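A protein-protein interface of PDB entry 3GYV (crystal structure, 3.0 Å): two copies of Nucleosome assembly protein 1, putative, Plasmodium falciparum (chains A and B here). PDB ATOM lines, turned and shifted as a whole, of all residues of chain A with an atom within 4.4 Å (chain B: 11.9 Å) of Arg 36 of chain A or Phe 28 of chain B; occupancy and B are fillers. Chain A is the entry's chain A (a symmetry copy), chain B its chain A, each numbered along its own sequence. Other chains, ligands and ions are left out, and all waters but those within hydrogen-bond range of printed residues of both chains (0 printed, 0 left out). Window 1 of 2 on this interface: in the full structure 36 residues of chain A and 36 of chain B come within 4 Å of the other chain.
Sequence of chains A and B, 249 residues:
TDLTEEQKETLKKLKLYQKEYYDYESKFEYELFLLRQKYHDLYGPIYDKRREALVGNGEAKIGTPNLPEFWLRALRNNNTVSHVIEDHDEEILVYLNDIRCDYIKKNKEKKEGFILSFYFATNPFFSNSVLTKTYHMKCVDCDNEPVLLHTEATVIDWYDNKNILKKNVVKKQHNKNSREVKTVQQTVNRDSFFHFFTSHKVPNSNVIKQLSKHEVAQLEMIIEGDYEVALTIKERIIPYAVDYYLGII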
ATOM      1  N   LEU A  32     -26.778   4.543   7.188  1.00  0.00           N
ATOM      2  CA  LEU A  32     -25.386   4.906   6.949  1.00  0.00           C
ATOM      3  C   LEU A  32     -24.368   3.940   7.601  1.00  0.00           C
ATOM      4  O   LEU A  32     -23.392   3.571   6.945  1.00  0.00           O
ATOM      5  CB  LEU A  32     -25.132   6.361   7.360  1.00  0.00           C
ATOM      6  CG  LEU A  32     -23.720   6.911   7.174  1.00  0.00           C
ATOM      7  CD1 LEU A  32     -23.309   6.833   5.718  1.00  0.00           C
ATOM      8  CD2 LEU A  32     -23.618   8.330   7.666  1.00  0.00           C
ATOM      9  N   PHE A  33     -24.586   3.538   8.866  1.00  0.00           N
ATOM     10  CA  PHE A  33     -23.743   2.518   9.532  1.00  0.00           C
ATOM     11  C   PHE A  33     -23.747   1.245   8.686  1.00  0.00           C
ATOM     12  O   PHE A  33     -22.692   0.687   8.384  1.00  0.00           O
ATOM     13  CB  PHE A  33     -24.252   2.108  10.932  1.00  0.00           C
ATOM     14  CG  PHE A  33     -24.259   3.209  11.977  1.00  0.00           C
ATOM     15  CD1 PHE A  33     -23.472   4.370  11.849  1.00  0.00           C
ATOM     16  CD2 PHE A  33     -25.049   3.056  13.141  1.00  0.00           C
ATOM     17  CE1 PHE A  33     -23.494   5.381  12.858  1.00  0.00           C
ATOM     18  CE2 PHE A  33     -25.080   4.048  14.154  1.00  0.00           C
ATOM     19  CZ  PHE A  33     -24.300   5.212  14.011  1.00  0.00           C
ATOM     20  N   LEU A  34     -24.956   0.794   8.337  1.00  0.00           N
ATOM     21  CA  LEU A  34     -25.174  -0.380   7.515  1.00  0.00           C
ATOM     22  C   LEU A  34     -24.335  -0.341   6.259  1.00  0.00           C
ATOM     23  O   LEU A  34     -23.615  -1.282   5.962  1.00  0.00           O
ATOM     24  CB  LEU A  34     -26.637  -0.463   7.107  1.00  0.00           C
ATOM     25  CG  LEU A  34     -27.605  -1.338   7.899  1.00  0.00           C
ATOM     26  CD1 LEU A  34     -29.050  -1.098   7.425  1.00  0.00           C
ATOM     27  CD2 LEU A  34     -27.239  -2.791   7.751  1.00  0.00           C
ATOM     28  N   LEU A  35     -24.432   0.757   5.519  1.00  0.00           N
ATOM     29  CA  LEU A  35     -23.705   0.906   4.267  1.00  0.00           C
ATOM     30  C   LEU A  35     -22.206   0.852   4.472  1.00  0.00           C
ATOM     31  O   LEU A  35     -21.517   0.224   3.681  1.00  0.00           O
ATOM     32  CB  LEU A  35     -24.085   2.203   3.552  1.00  0.00           C
ATOM     33  CG  LEU A  35     -23.868   2.268   2.038  1.00  0.00           C
ATOM     34  CD1 LEU A  35     -24.389   1.024   1.314  1.00  0.00           C
ATOM     35  CD2 LEU A  35     -24.530   3.515   1.488  1.00  0.00           C
ATOM     36  N   ARG A  36     -21.700   1.498   5.523  1.00  0.00           N
ATOM     37  CA  ARG A  36     -20.264   1.466   5.815  1.00  0.00           C
ATOM     38  C   ARG A  36     -19.747   0.073   6.192  1.00  0.00           C
ATOM     39  O   ARG A  36     -18.715  -0.369   5.683  1.00  0.00           O
ATOM     40  CB  ARG A  36     -19.887   2.496   6.875  1.00  0.00           C
ATOM     41  CG  ARG A  36     -19.838   3.891   6.327  1.00  0.00           C
ATOM     42  CD  ARG A  36     -19.014   4.830   7.180  1.00  0.00           C
ATOM     43  NE  ARG A  36     -19.332   6.231   6.870  1.00  0.00           N
ATOM     44  CZ  ARG A  36     -18.826   6.929   5.847  1.00  0.00           C
ATOM     45  NH1 ARG A  36     -17.952   6.369   5.011  1.00  0.00           N
ATOM     46  NH2 ARG A  36     -19.196   8.192   5.656  1.00  0.00           N
ATOM     47  N   GLN A  37     -20.479  -0.621   7.059  1.00  0.00           N
ATOM     48  CA  GLN A  37     -20.144  -2.000   7.413  1.00  0.00           C
ATOM     49  C   GLN A  37     -20.200  -2.939   6.208  1.00  0.00           C
ATOM     50  O   GLN A  37     -19.267  -3.719   5.990  1.00  0.00           O
ATOM     51  CB  GLN A  37     -21.018  -2.532   8.571  1.00  0.00           C
ATOM     52  CG  GLN A  37     -20.977  -1.685   9.878  1.00  0.00           C
ATOM     53  CD  GLN A  37     -19.562  -1.402  10.420  1.00  0.00           C
ATOM     54  OE1 GLN A  37     -18.874  -0.475   9.969  1.00  0.00           O
ATOM     55  NE2 GLN A  37     -19.148  -2.179  11.416  1.00  0.00           N
ATOM     56  N   LYS A  38     -21.275  -2.856   5.427  1.00  0.00           N
ATOM     57  CA  LYS A  38     -21.384  -3.613   4.176  1.00  0.00           C
ATOM     58  C   LYS A  38     -20.099  -3.525   3.354  1.00  0.00           C
ATOM     59  O   LYS A  38     -19.590  -4.538   2.883  1.00  0.00           O
ATOM     60  CB  LYS A  38     -22.583  -3.128   3.348  1.00  0.00           C
ATOM     61  CG  LYS A  38     -22.855  -3.917   2.066  1.00  0.00           C
ATOM     62  CD  LYS A  38     -24.067  -3.366   1.346  1.00  0.00           C
ATOM     63  CE  LYS A  38     -24.303  -4.051   0.019  1.00  0.00           C
ATOM     64  NZ  LYS A  38     -24.722  -3.074  -1.044  1.00  0.00           N
ATOM     65  N   TYR A  39     -19.563  -2.313   3.223  1.00  0.00           N
ATOM     66  CA  TYR A  39     -18.390  -2.073   2.391  1.00  0.00           C
ATOM     67  C   TYR A  39     -17.023  -2.330   3.045  1.00  0.00           C
ATOM     68  O   TYR A  39     -16.096  -2.773   2.374  1.00  0.00           O
ATOM     69  CB  TYR A  39     -18.499  -0.716   1.704  1.00  0.00           C
ATOM     70  CG  TYR A  39     -19.418  -0.810   0.511  1.00  0.00           C
ATOM     71  CD1 TYR A  39     -18.904  -0.965  -0.778  1.00  0.00           C
ATOM     72  CD2 TYR A  39     -20.807  -0.805   0.671  1.00  0.00           C
ATOM     73  CE1 TYR A  39     -19.756  -1.084  -1.892  1.00  0.00           C
ATOM     74  CE2 TYR A  39     -21.666  -0.918  -0.434  1.00  0.00           C
ATOM     75  CZ  TYR A  39     -21.130  -1.057  -1.712  1.00  0.00           C
ATOM     76  OH  TYR A  39     -21.966  -1.180  -2.799  1.00  0.00           O
ATOM     77  N   HIS A  40     -16.903  -2.094   4.346  1.00  0.00           N
ATOM     78  CA  HIS A  40     -15.737  -2.557   5.101  1.00  0.00           C
ATOM     79  C   HIS A  40     -15.506  -4.074   4.898  1.00  0.00           C
ATOM     80  O   HIS A  40     -14.374  -4.535   4.756  1.00  0.00           O
ATOM     81  CB  HIS A  40     -15.928  -2.208   6.580  1.00  0.00           C
ATOM     82  CG  HIS A  40     -14.772  -2.589   7.456  1.00  0.00           C
ATOM     83  ND1 HIS A  40     -13.713  -1.738   7.703  1.00  0.00           N
ATOM     84  CD2 HIS A  40     -14.514  -3.723   8.153  1.00  0.00           C
ATOM     85  CE1 HIS A  40     -12.849  -2.334   8.509  1.00  0.00           C
ATOM     86  NE2 HIS A  40     -13.312  -3.538   8.798  1.00  0.00           N
ATOM     87  N   TYR A  43     -14.312  -4.630   1.252  1.00  0.00           N
ATOM     88  CA  TYR A  43     -12.891  -4.337   1.111  1.00  0.00           C
ATOM     89  C   TYR A  43     -12.038  -5.467   1.698  1.00  0.00           C
ATOM     90  O   TYR A  43     -11.171  -6.023   1.007  1.00  0.00           O
ATOM     91  CB  TYR A  43     -12.545  -2.976   1.727  1.00  0.00           C
ATOM     92  CG  TYR A  43     -13.402  -1.854   1.187  1.00  0.00           C
ATOM     93  CD1 TYR A  43     -13.719  -1.792  -0.176  1.00  0.00           C
ATOM     94  CD2 TYR A  43     -13.897  -0.855   2.021  1.00  0.00           C
ATOM     95  CE1 TYR A  43     -14.518  -0.768  -0.694  1.00  0.00           C
ATOM     96  CE2 TYR A  43     -14.704   0.177   1.505  1.00  0.00           C
ATOM     97  CZ  TYR A  43     -15.006   0.206   0.149  1.00  0.00           C
ATOM     98  OH  TYR A  43     -15.796   1.193  -0.383  1.00  0.00           O
ATOM     99  N   LYS B  19      -8.111  -2.040  -8.872  1.00  0.00           N
ATOM    100  CA  LYS B  19      -9.231  -1.753  -9.786  1.00  0.00           C
ATOM    101  C   LYS B  19     -10.469  -2.284  -9.126  1.00  0.00           C
ATOM    102  O   LYS B  19     -11.468  -1.571  -9.010  1.00  0.00           O
ATOM    103  CB  LYS B  19      -9.104  -2.475 -11.130  1.00  0.00           C
ATOM    104  CG  LYS B  19      -7.997  -2.001 -12.029  1.00  0.00           C
ATOM    105  CD  LYS B  19      -7.490  -3.166 -12.897  1.00  0.00           C
ATOM    106  CE  LYS B  19      -6.216  -2.827 -13.714  1.00  0.00           C
ATOM    107  NZ  LYS B  19      -5.762  -3.981 -14.573  1.00  0.00           N
ATOM    108  N   GLU B  20     -10.391  -3.540  -8.689  1.00  0.00           N
ATOM    109  CA  GLU B  20     -11.505  -4.190  -8.014  1.00  0.00           C
ATOM    110  C   GLU B  20     -12.023  -3.319  -6.861  1.00  0.00           C
ATOM    111  O   GLU B  20     -13.221  -3.062  -6.749  1.00  0.00           O
ATOM    112  CB  GLU B  20     -11.100  -5.577  -7.511  1.00  0.00           C
ATOM    113  CG  GLU B  20     -12.305  -6.413  -7.096  1.00  0.00           C
ATOM    114  CD  GLU B  20     -11.937  -7.700  -6.374  1.00  0.00           C
ATOM    115  OE1 GLU B  20     -10.721  -7.996  -6.263  1.00  0.00           O
ATOM    116  OE2 GLU B  20     -12.868  -8.418  -5.923  1.00  0.00           O
ATOM    117  N   TYR B  21     -11.087  -2.857  -6.034  1.00  0.00           N
ATOM    118  CA  TYR B  21     -11.364  -1.908  -4.978  1.00  0.00           C
ATOM    119  C   TYR B  21     -12.157  -0.722  -5.502  1.00  0.00           C
ATOM    120  O   TYR B  21     -13.208  -0.392  -4.949  1.00  0.00           O
ATOM    121  CB  TYR B  21     -10.073  -1.402  -4.322  1.00  0.00           C
ATOM    122  CG  TYR B  21     -10.392  -0.423  -3.240  1.00  0.00           C
ATOM    123  CD1 TYR B  21     -10.603  -0.860  -1.937  1.00  0.00           C
ATOM    124  CD2 TYR B  21     -10.558   0.939  -3.529  1.00  0.00           C
ATOM    125  CE1 TYR B  21     -10.930   0.032  -0.930  1.00  0.00           C
ATOM    126  CE2 TYR B  21     -10.900   1.847  -2.536  1.00  0.00           C
ATOM    127  CZ  TYR B  21     -11.084   1.385  -1.235  1.00  0.00           C
ATOM    128  OH  TYR B  21     -11.427   2.260  -0.225  1.00  0.00           O
ATOM    129  N   TYR B  22     -11.652  -0.084  -6.561  1.00  0.00           N
ATOM    130  CA  TYR B  22     -12.316   1.074  -7.156  1.00  0.00           C
ATOM    131  C   TYR B  22     -13.719   0.784  -7.626  1.00  0.00           C
ATOM    132  O   TYR B  22     -14.556   1.680  -7.629  1.00  0.00           O
ATOM    133  CB  TYR B  22     -11.493   1.685  -8.294  1.00  0.00           C
ATOM    134  CG  TYR B  22     -10.273   2.437  -7.799  1.00  0.00           C
ATOM    135  CD1 TYR B  22     -10.325   3.181  -6.615  1.00  0.00           C
ATOM    136  CD2 TYR B  22      -9.070   2.403  -8.501  1.00  0.00           C
ATOM    137  CE1 TYR B  22      -9.211   3.862  -6.142  1.00  0.00           C
ATOM    138  CE2 TYR B  22      -7.951   3.079  -8.032  1.00  0.00           C
ATOM    139  CZ  TYR B  22      -8.033   3.806  -6.857  1.00  0.00           C
ATOM    140  OH  TYR B  22      -6.941   4.484  -6.387  1.00  0.00           O
ATOM    141  N   ASP B  23     -13.986  -0.466  -7.995  1.00  0.00           N
ATOM    142  CA  ASP B  23     -15.330  -0.848  -8.399  1.00  0.00           C
ATOM    143  C   ASP B  23     -16.303  -0.778  -7.243  1.00  0.00           C
ATOM    144  O   ASP B  23     -17.442  -0.333  -7.418  1.00  0.00           O
ATOM    145  CB  ASP B  23     -15.358  -2.239  -9.014  1.00  0.00           C
ATOM    146  CG  ASP B  23     -14.490  -2.354 -10.260  1.00  0.00           C
ATOM    147  OD1 ASP B  23     -14.421  -1.378 -11.065  1.00  0.00           O
ATOM    148  OD2 ASP B  23     -13.882  -3.449 -10.421  1.00  0.00           O
ATOM    149  N   TYR B  24     -15.846  -1.216  -6.068  1.00  0.00           N
ATOM    150  CA  TYR B  24     -16.660  -1.216  -4.862  1.00  0.00           C
ATOM    151  C   TYR B  24     -16.820   0.186  -4.288  1.00  0.00           C
ATOM    152  O   TYR B  24     -17.916   0.576  -3.912  1.00  0.00           O
ATOM    153  CB  TYR B  24     -16.077  -2.148  -3.813  1.00  0.00           C
ATOM    154  CG  TYR B  24     -16.343  -3.608  -4.064  1.00  0.00           C
ATOM    155  CD1 TYR B  24     -17.648  -4.094  -4.142  1.00  0.00           C
ATOM    156  CD2 TYR B  24     -15.286  -4.516  -4.200  1.00  0.00           C
ATOM    157  CE1 TYR B  24     -17.902  -5.456  -4.372  1.00  0.00           C
ATOM    158  CE2 TYR B  24     -15.520  -5.876  -4.436  1.00  0.00           C
ATOM    159  CZ  TYR B  24     -16.830  -6.339  -4.520  1.00  0.00           C
ATOM    160  OH  TYR B  24     -17.074  -7.674  -4.748  1.00  0.00           O
ATOM    161  N   GLU B  25     -15.736   0.950  -4.228  1.00  0.00           N
ATOM    162  CA  GLU B  25     -15.823   2.342  -3.805  1.00  0.00           C
ATOM    163  C   GLU B  25     -16.806   3.092  -4.721  1.00  0.00           C
ATOM    164  O   GLU B  25     -17.470   4.047  -4.297  1.00  0.00           O
ATOM    165  CB  GLU B  25     -14.440   2.994  -3.812  1.00  0.00           C
ATOM    166  CG  GLU B  25     -14.450   4.469  -3.517  1.00  0.00           C
ATOM    167  CD  GLU B  25     -13.077   5.030  -3.195  1.00  0.00           C
ATOM    168  OE1 GLU B  25     -12.136   4.846  -3.989  1.00  0.00           O
ATOM    169  OE2 GLU B  25     -12.931   5.683  -2.144  1.00  0.00           O
ATOM    170  N   SER B  26     -16.904   2.646  -5.972  1.00  0.00           N
ATOM    171  CA  SER B  26     -17.861   3.220  -6.903  1.00  0.00           C
ATOM    172  C   SER B  26     -19.277   2.954  -6.437  1.00  0.00           C
ATOM    173  O   SER B  26     -20.054   3.894  -6.241  1.00  0.00           O
ATOM    174  CB  SER B  26     -17.672   2.665  -8.313  1.00  0.00           C
ATOM    175  OG  SER B  26     -16.997   3.605  -9.117  1.00  0.00           O
ATOM    176  N   LYS B  27     -19.596   1.670  -6.269  1.00  0.00           N
ATOM    177  CA  LYS B  27     -20.913   1.244  -5.820  1.00  0.00           C
ATOM    178  C   LYS B  27     -21.272   1.917  -4.508  1.00  0.00           C
ATOM    179  O   LYS B  27     -22.414   2.300  -4.296  1.00  0.00           O
ATOM    180  CB  LYS B  27     -20.969  -0.275  -5.677  1.00  0.00           C
ATOM    181  CG  LYS B  27     -21.177  -0.984  -6.989  1.00  0.00           C
ATOM    182  CD  LYS B  27     -20.801  -2.456  -6.896  1.00  0.00           C
ATOM    183  CE  LYS B  27     -20.821  -3.122  -8.276  1.00  0.00           C
ATOM    184  NZ  LYS B  27     -19.848  -2.510  -9.241  1.00  0.00           N
ATOM    185  N   PHE B  28     -20.274   2.080  -3.647  1.00  0.00           N
ATOM    186  CA  PHE B  28     -20.435   2.760  -2.377  1.00  0.00           C
ATOM    187  C   PHE B  28     -20.970   4.161  -2.571  1.00  0.00           C
ATOM    188  O   PHE B  28     -22.129   4.427  -2.287  1.00  0.00           O
ATOM    189  CB  PHE B  28     -19.107   2.822  -1.624  1.00  0.00           C
ATOM    190  CG  PHE B  28     -19.209   3.498  -0.298  1.00  0.00           C
ATOM    191  CD1 PHE B  28     -19.943   2.915   0.737  1.00  0.00           C
ATOM    192  CD2 PHE B  28     -18.587   4.732  -0.083  1.00  0.00           C
ATOM    193  CE1 PHE B  28     -20.056   3.549   1.980  1.00  0.00           C
ATOM    194  CE2 PHE B  28     -18.681   5.379   1.160  1.00  0.00           C
ATOM    195  CZ  PHE B  28     -19.418   4.784   2.196  1.00  0.00           C
ATOM    196  N   GLU B  29     -20.121   5.055  -3.060  1.00  0.00           N
ATOM    197  CA  GLU B  29     -20.530   6.436  -3.340  1.00  0.00           C
ATOM    198  C   GLU B  29     -21.890   6.561  -4.033  1.00  0.00           C
ATOM    199  O   GLU B  29     -22.656   7.471  -3.727  1.00  0.00           O
ATOM    200  CB  GLU B  29     -19.472   7.144  -4.171  1.00  0.00           C
ATOM    201  CG  GLU B  29     -18.255   7.584  -3.390  1.00  0.00           C
ATOM    202  CD  GLU B  29     -17.140   8.002  -4.315  1.00  0.00           C
ATOM    203  OE1 GLU B  29     -17.428   8.756  -5.275  1.00  0.00           O
ATOM    204  OE2 GLU B  29     -15.984   7.569  -4.100  1.00  0.00           O
ATOM    205  N   TYR B  30     -22.176   5.650  -4.963  1.00  0.00           N
ATOM    206  CA  TYR B  30     -23.479   5.593  -5.605  1.00  0.00           C
ATOM    207  C   TYR B  30     -24.580   5.309  -4.594  1.00  0.00           C
ATOM    208  O   TYR B  30     -25.559   6.053  -4.522  1.00  0.00           O
ATOM    209  CB  TYR B  30     -23.509   4.542  -6.707  1.00  0.00           C
ATOM    210  CG  TYR B  30     -24.836   4.494  -7.429  1.00  0.00           C
ATOM    211  CD1 TYR B  30     -25.192   5.503  -8.330  1.00  0.00           C
ATOM    212  CD2 TYR B  30     -25.741   3.446  -7.213  1.00  0.00           C
ATOM    213  CE1 TYR B  30     -26.411   5.472  -9.001  1.00  0.00           C
ATOM    214  CE2 TYR B  30     -26.966   3.402  -7.880  1.00  0.00           C
ATOM    215  CZ  TYR B  30     -27.297   4.421  -8.773  1.00  0.00           C
ATOM    216  OH  TYR B  30     -28.507   4.408  -9.444  1.00  0.00           O
ATOM    217  N   GLU B  31     -24.413   4.239  -3.816  1.00  0.00           N
ATOM    218  CA  GLU B  31     -25.350   3.913  -2.727  1.00  0.00           C
ATOM    219  C   GLU B  31     -25.409   5.003  -1.648  1.00  0.00           C
ATOM    220  O   GLU B  31     -26.443   5.170  -0.993  1.00  0.00           O
ATOM    221  CB  GLU B  31     -25.026   2.567  -2.096  1.00  0.00           C
ATOM    222  CG  GLU B  31     -25.064   1.451  -3.079  1.00  0.00           C
ATOM    223  CD  GLU B  31     -25.829   0.287  -2.556  1.00  0.00           C
ATOM    224  OE1 GLU B  31     -27.034   0.203  -2.883  1.00  0.00           O
ATOM    225  OE2 GLU B  31     -25.239  -0.527  -1.809  1.00  0.00           O
ATOM    226  N   LEU B  32     -24.305   5.736  -1.487  1.00  0.00           N
ATOM    227  CA  LEU B  32     -24.251   6.910  -0.625  1.00  0.00           C
ATOM    228  C   LEU B  32     -25.034   8.126  -1.176  1.00  0.00           C
ATOM    229  O   LEU B  32     -25.751   8.770  -0.408  1.00  0.00           O
ATOM    230  CB  LEU B  32     -22.797   7.271  -0.300  1.00  0.00           C
ATOM    231  CG  LEU B  32     -22.555   8.481   0.599  1.00  0.00           C
ATOM    232  CD1 LEU B  32     -23.224   8.283   1.944  1.00  0.00           C
ATOM    233  CD2 LEU B  32     -21.083   8.736   0.786  1.00  0.00           C
ATOM    234  N   PHE B  33     -24.903   8.436  -2.479  1.00  0.00           N
ATOM    235  CA  PHE B  33     -25.707   9.497  -3.128  1.00  0.00           C
ATOM    236  C   PHE B  33     -27.189   9.188  -2.923  1.00  0.00           C
ATOM    237  O   PHE B  33     -27.958  10.051  -2.497  1.00  0.00           O
ATOM    238  CB  PHE B  33     -25.493   9.593  -4.655  1.00  0.00           C
ATOM    239  CG  PHE B  33     -24.092   9.975  -5.098  1.00  0.00           C
ATOM    240  CD1 PHE B  33     -23.182  10.620  -4.238  1.00  0.00           C
ATOM    241  CD2 PHE B  33     -23.691   9.714  -6.430  1.00  0.00           C
ATOM    242  CE1 PHE B  33     -21.874  10.975  -4.694  1.00  0.00           C
ATOM    243  CE2 PHE B  33     -22.399  10.064  -6.899  1.00  0.00           C
ATOM    244  CZ  PHE B  33     -21.490  10.695  -6.028  1.00  0.00           C
ATOM    245  N   LEU B  34     -27.568   7.951  -3.258  1.00  0.00           N
ATOM    246  CA  LEU B  34     -28.922   7.453  -3.115  1.00  0.00           C
ATOM    247  C   LEU B  34     -29.468   7.725  -1.732  1.00  0.00           C
ATOM    248  O   LEU B  34     -30.541   8.291  -1.588  1.00  0.00           O
ATOM    249  CB  LEU B  34     -28.949   5.951  -3.349  1.00  0.00           C
ATOM    250  CG  LEU B  34     -29.325   5.396  -4.721  1.00  0.00           C
ATOM    251  CD1 LEU B  34     -29.084   3.877  -4.765  1.00  0.00           C
ATOM    252  CD2 LEU B  34     -30.764   5.708  -5.036  1.00  0.00           C
ATOM    253  N   LEU B  35     -28.722   7.317  -0.712  1.00  0.00           N
ATOM    254  CA  LEU B  35     -29.151   7.486   0.668  1.00  0.00           C
ATOM    255  C   LEU B  35     -29.329   8.944   1.033  1.00  0.00           C
ATOM    256  O   LEU B  35     -30.295   9.278   1.705  1.00  0.00           O
ATOM    257  CB  LEU B  35     -28.174   6.823   1.641  1.00  0.00           C
ATOM    258  CG  LEU B  35     -28.708   6.421   3.018  1.00  0.00           C
ATOM    259  CD1 LEU B  35     -30.048   5.686   2.940  1.00  0.00           C
ATOM    260  CD2 LEU B  35     -27.678   5.566   3.727  1.00  0.00           C
ATOM    261  N   ARG B  36     -28.415   9.809   0.594  1.00  0.00           N
ATOM    262  CA  ARG B  36     -28.532  11.244   0.871  1.00  0.00           C
ATOM    263  C   ARG B  36     -29.742  11.901   0.196  1.00  0.00           C
ATOM    264  O   ARG B  36     -30.478  12.657   0.832  1.00  0.00           O
ATOM    265  CB  ARG B  36     -27.244  11.986   0.530  1.00  0.00           C
ATOM    266  CG  ARG B  36     -26.174  11.781   1.560  1.00  0.00           C
ATOM    267  CD  ARG B  36     -25.107  12.853   1.523  1.00  0.00           C
ATOM    268  NE  ARG B  36     -23.893  12.405   2.219  1.00  0.00           N
ATOM    269  CZ  ARG B  36     -23.702  12.448   3.543  1.00  0.00           C
ATOM    270  NH1 ARG B  36     -24.647  12.932   4.348  1.00  0.00           N
ATOM    271  NH2 ARG B  36     -22.563  12.002   4.065  1.00  0.00           N
ATOM    272  N   GLN B  37     -29.955  11.588  -1.079  1.00  0.00           N
ATOM    273  CA  GLN B  37     -31.135  12.069  -1.798  1.00  0.00           C
ATOM    274  C   GLN B  37     -32.438  11.563  -1.179  1.00  0.00           C
ATOM    275  O   GLN B  37     -33.363  12.351  -0.957  1.00  0.00           O
ATOM    276  CB  GLN B  37     -31.073  11.737  -3.306  1.00  0.00           C
ATOM    277  CG  GLN B  37     -29.815  12.273  -4.053  1.00  0.00           C
ATOM    278  CD  GLN B  37     -29.547  13.779  -3.868  1.00  0.00           C
ATOM    279  OE1 GLN B  37     -28.958  14.210  -2.867  1.00  0.00           O
ATOM    280  NE2 GLN B  37     -29.946  14.572  -4.858  1.00  0.00           N
ATOM    281  N   GLU B 235     -26.108  22.795   7.563  1.00  0.00           N
ATOM    282  CA  GLU B 235     -26.099  21.523   8.289  1.00  0.00           C
ATOM    283  C   GLU B 235     -26.499  21.583   9.758  1.00  0.00           C
ATOM    284  O   GLU B 235     -26.934  20.582  10.328  1.00  0.00           O
ATOM    285  CB  GLU B 235     -24.727  20.873   8.183  1.00  0.00           C
ATOM    286  CG  GLU B 235     -24.486  20.189   6.869  1.00  0.00           C
ATOM    287  CD  GLU B 235     -23.095  19.589   6.778  1.00  0.00           C
ATOM    288  OE1 GLU B 235     -22.204  20.011   7.564  1.00  0.00           O
ATOM    289  OE2 GLU B 235     -22.895  18.695   5.917  1.00  0.00           O
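Of the 20 printed residues of chain B, 8 touch a printed residue of chain A. Hydrophobic or aromatic side chains of chain B within 4 Å of the printed part of chain A: Tyr 21, Tyr 24, Phe 28 and Leu 35. Of the 10 printed residues of chain A, 6 touch a printed residue of chain B. Printed residues of chain A that touch a printed residue of chain B: Leu 32, Leu 35, Arg 36, Lys 38, Tyr 39 and Tyr 43. Hydrophobic or aromatic side chains of chain A within 4 Å of the printed part of chain B: Leu 35, Tyr 39 and Tyr 43. Among the printed residues, 13 pairs touch across the chains. Among the printed residues, Asp or Glu carboxylates within 4 Å of a Lys or Arg side-chain nitrogen of the other chain: Lys 38 of chain A with Glu 31 of chain B.
Leu 32 of chain A touches Leu 35 of chain B, and with the chains exchanged Leu 35 of chain A touches Leu 32 of chain B. Positions printed for both chains: 32, 33, 34, 35, 36 and 37. Of the 13 pairs that touch across the chains among the printed residues, 2 have their exchanged pair printed and touching as well.
The side-chain carboxylate of Glu 31 of chain B lies within salt-bridge range of the side-chain amino group of Lys 38 of chain A (2.7 Å). OE2 of Glu 31 of chain B is in hydrogen-bond range of OH of Tyr 39 of chain A, at 3.5 Å.
Glu 31 of chain B touches Leu 35 of chain A (O to CD2, 3.5 Å). Leu 35 of chain A touches Leu 32 of chain B (CD2 to N, 3.7 Å). Phe 28 of chain B touches Arg 36 of chain A. CE1 of Tyr 39 of chain A touches O of Tyr 24 of chain B, 3.2 Å away. CB of Lys 27 of chain B touches OH of Tyr 39 of chain A, at 3.2 Å. N of Phe 28 of chain B touches CE1 of Tyr 39 of chain A (3.7 Å). Tyr 43 of chain A touches Tyr 21 of chain B (CD1 to CE1, 3.4 Å). Tyr 24 of chain B touches Tyr 43 of chain A. OH of Tyr 43 of chain A touches CA of Glu 25 of chain B, 3.6 Å away. Tyr 43 of chain A touches Phe 28 of chain B.
Of chain B, only Leu 35 (3.7 Å) comes within 4 Å of Leu 32 of chain A. Printed residues of chain B within 4 Å of Leu 35 of chain A: Glu 31 and Leu 32. Of chain B, only Phe 28 (3.5 Å) comes within 4 Å of Arg 36 of chain A. No residue of chain B comes within 4 Å of Gln 37 of chain A. Tyr 39 of chain A touches just these residues of chain B: Tyr 24 (3.2 Å), Lys 27 (3.2 Å), Phe 28 (3.7 Å) and Glu 31 (3.5 Å). No residue of chain B comes within 4 Å of His 40 of chain A. Printed residues of chain A within 4 Å of Tyr 21 of chain B: Tyr 43 (3.4 Å). Of the printed residues of chain A, Leu 35 of chain B touches Leu 32. Gln 37 of chain B touches none of the printed residues of chain A. The nearest residue of chain B that does not touch Arg 36 of chain A is Leu 32 of chain B (5.3 Å). The nearest printed residue of chain A that does not touch Phe 28 of chain B is Leu 35 of chain A (4.01 Å).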
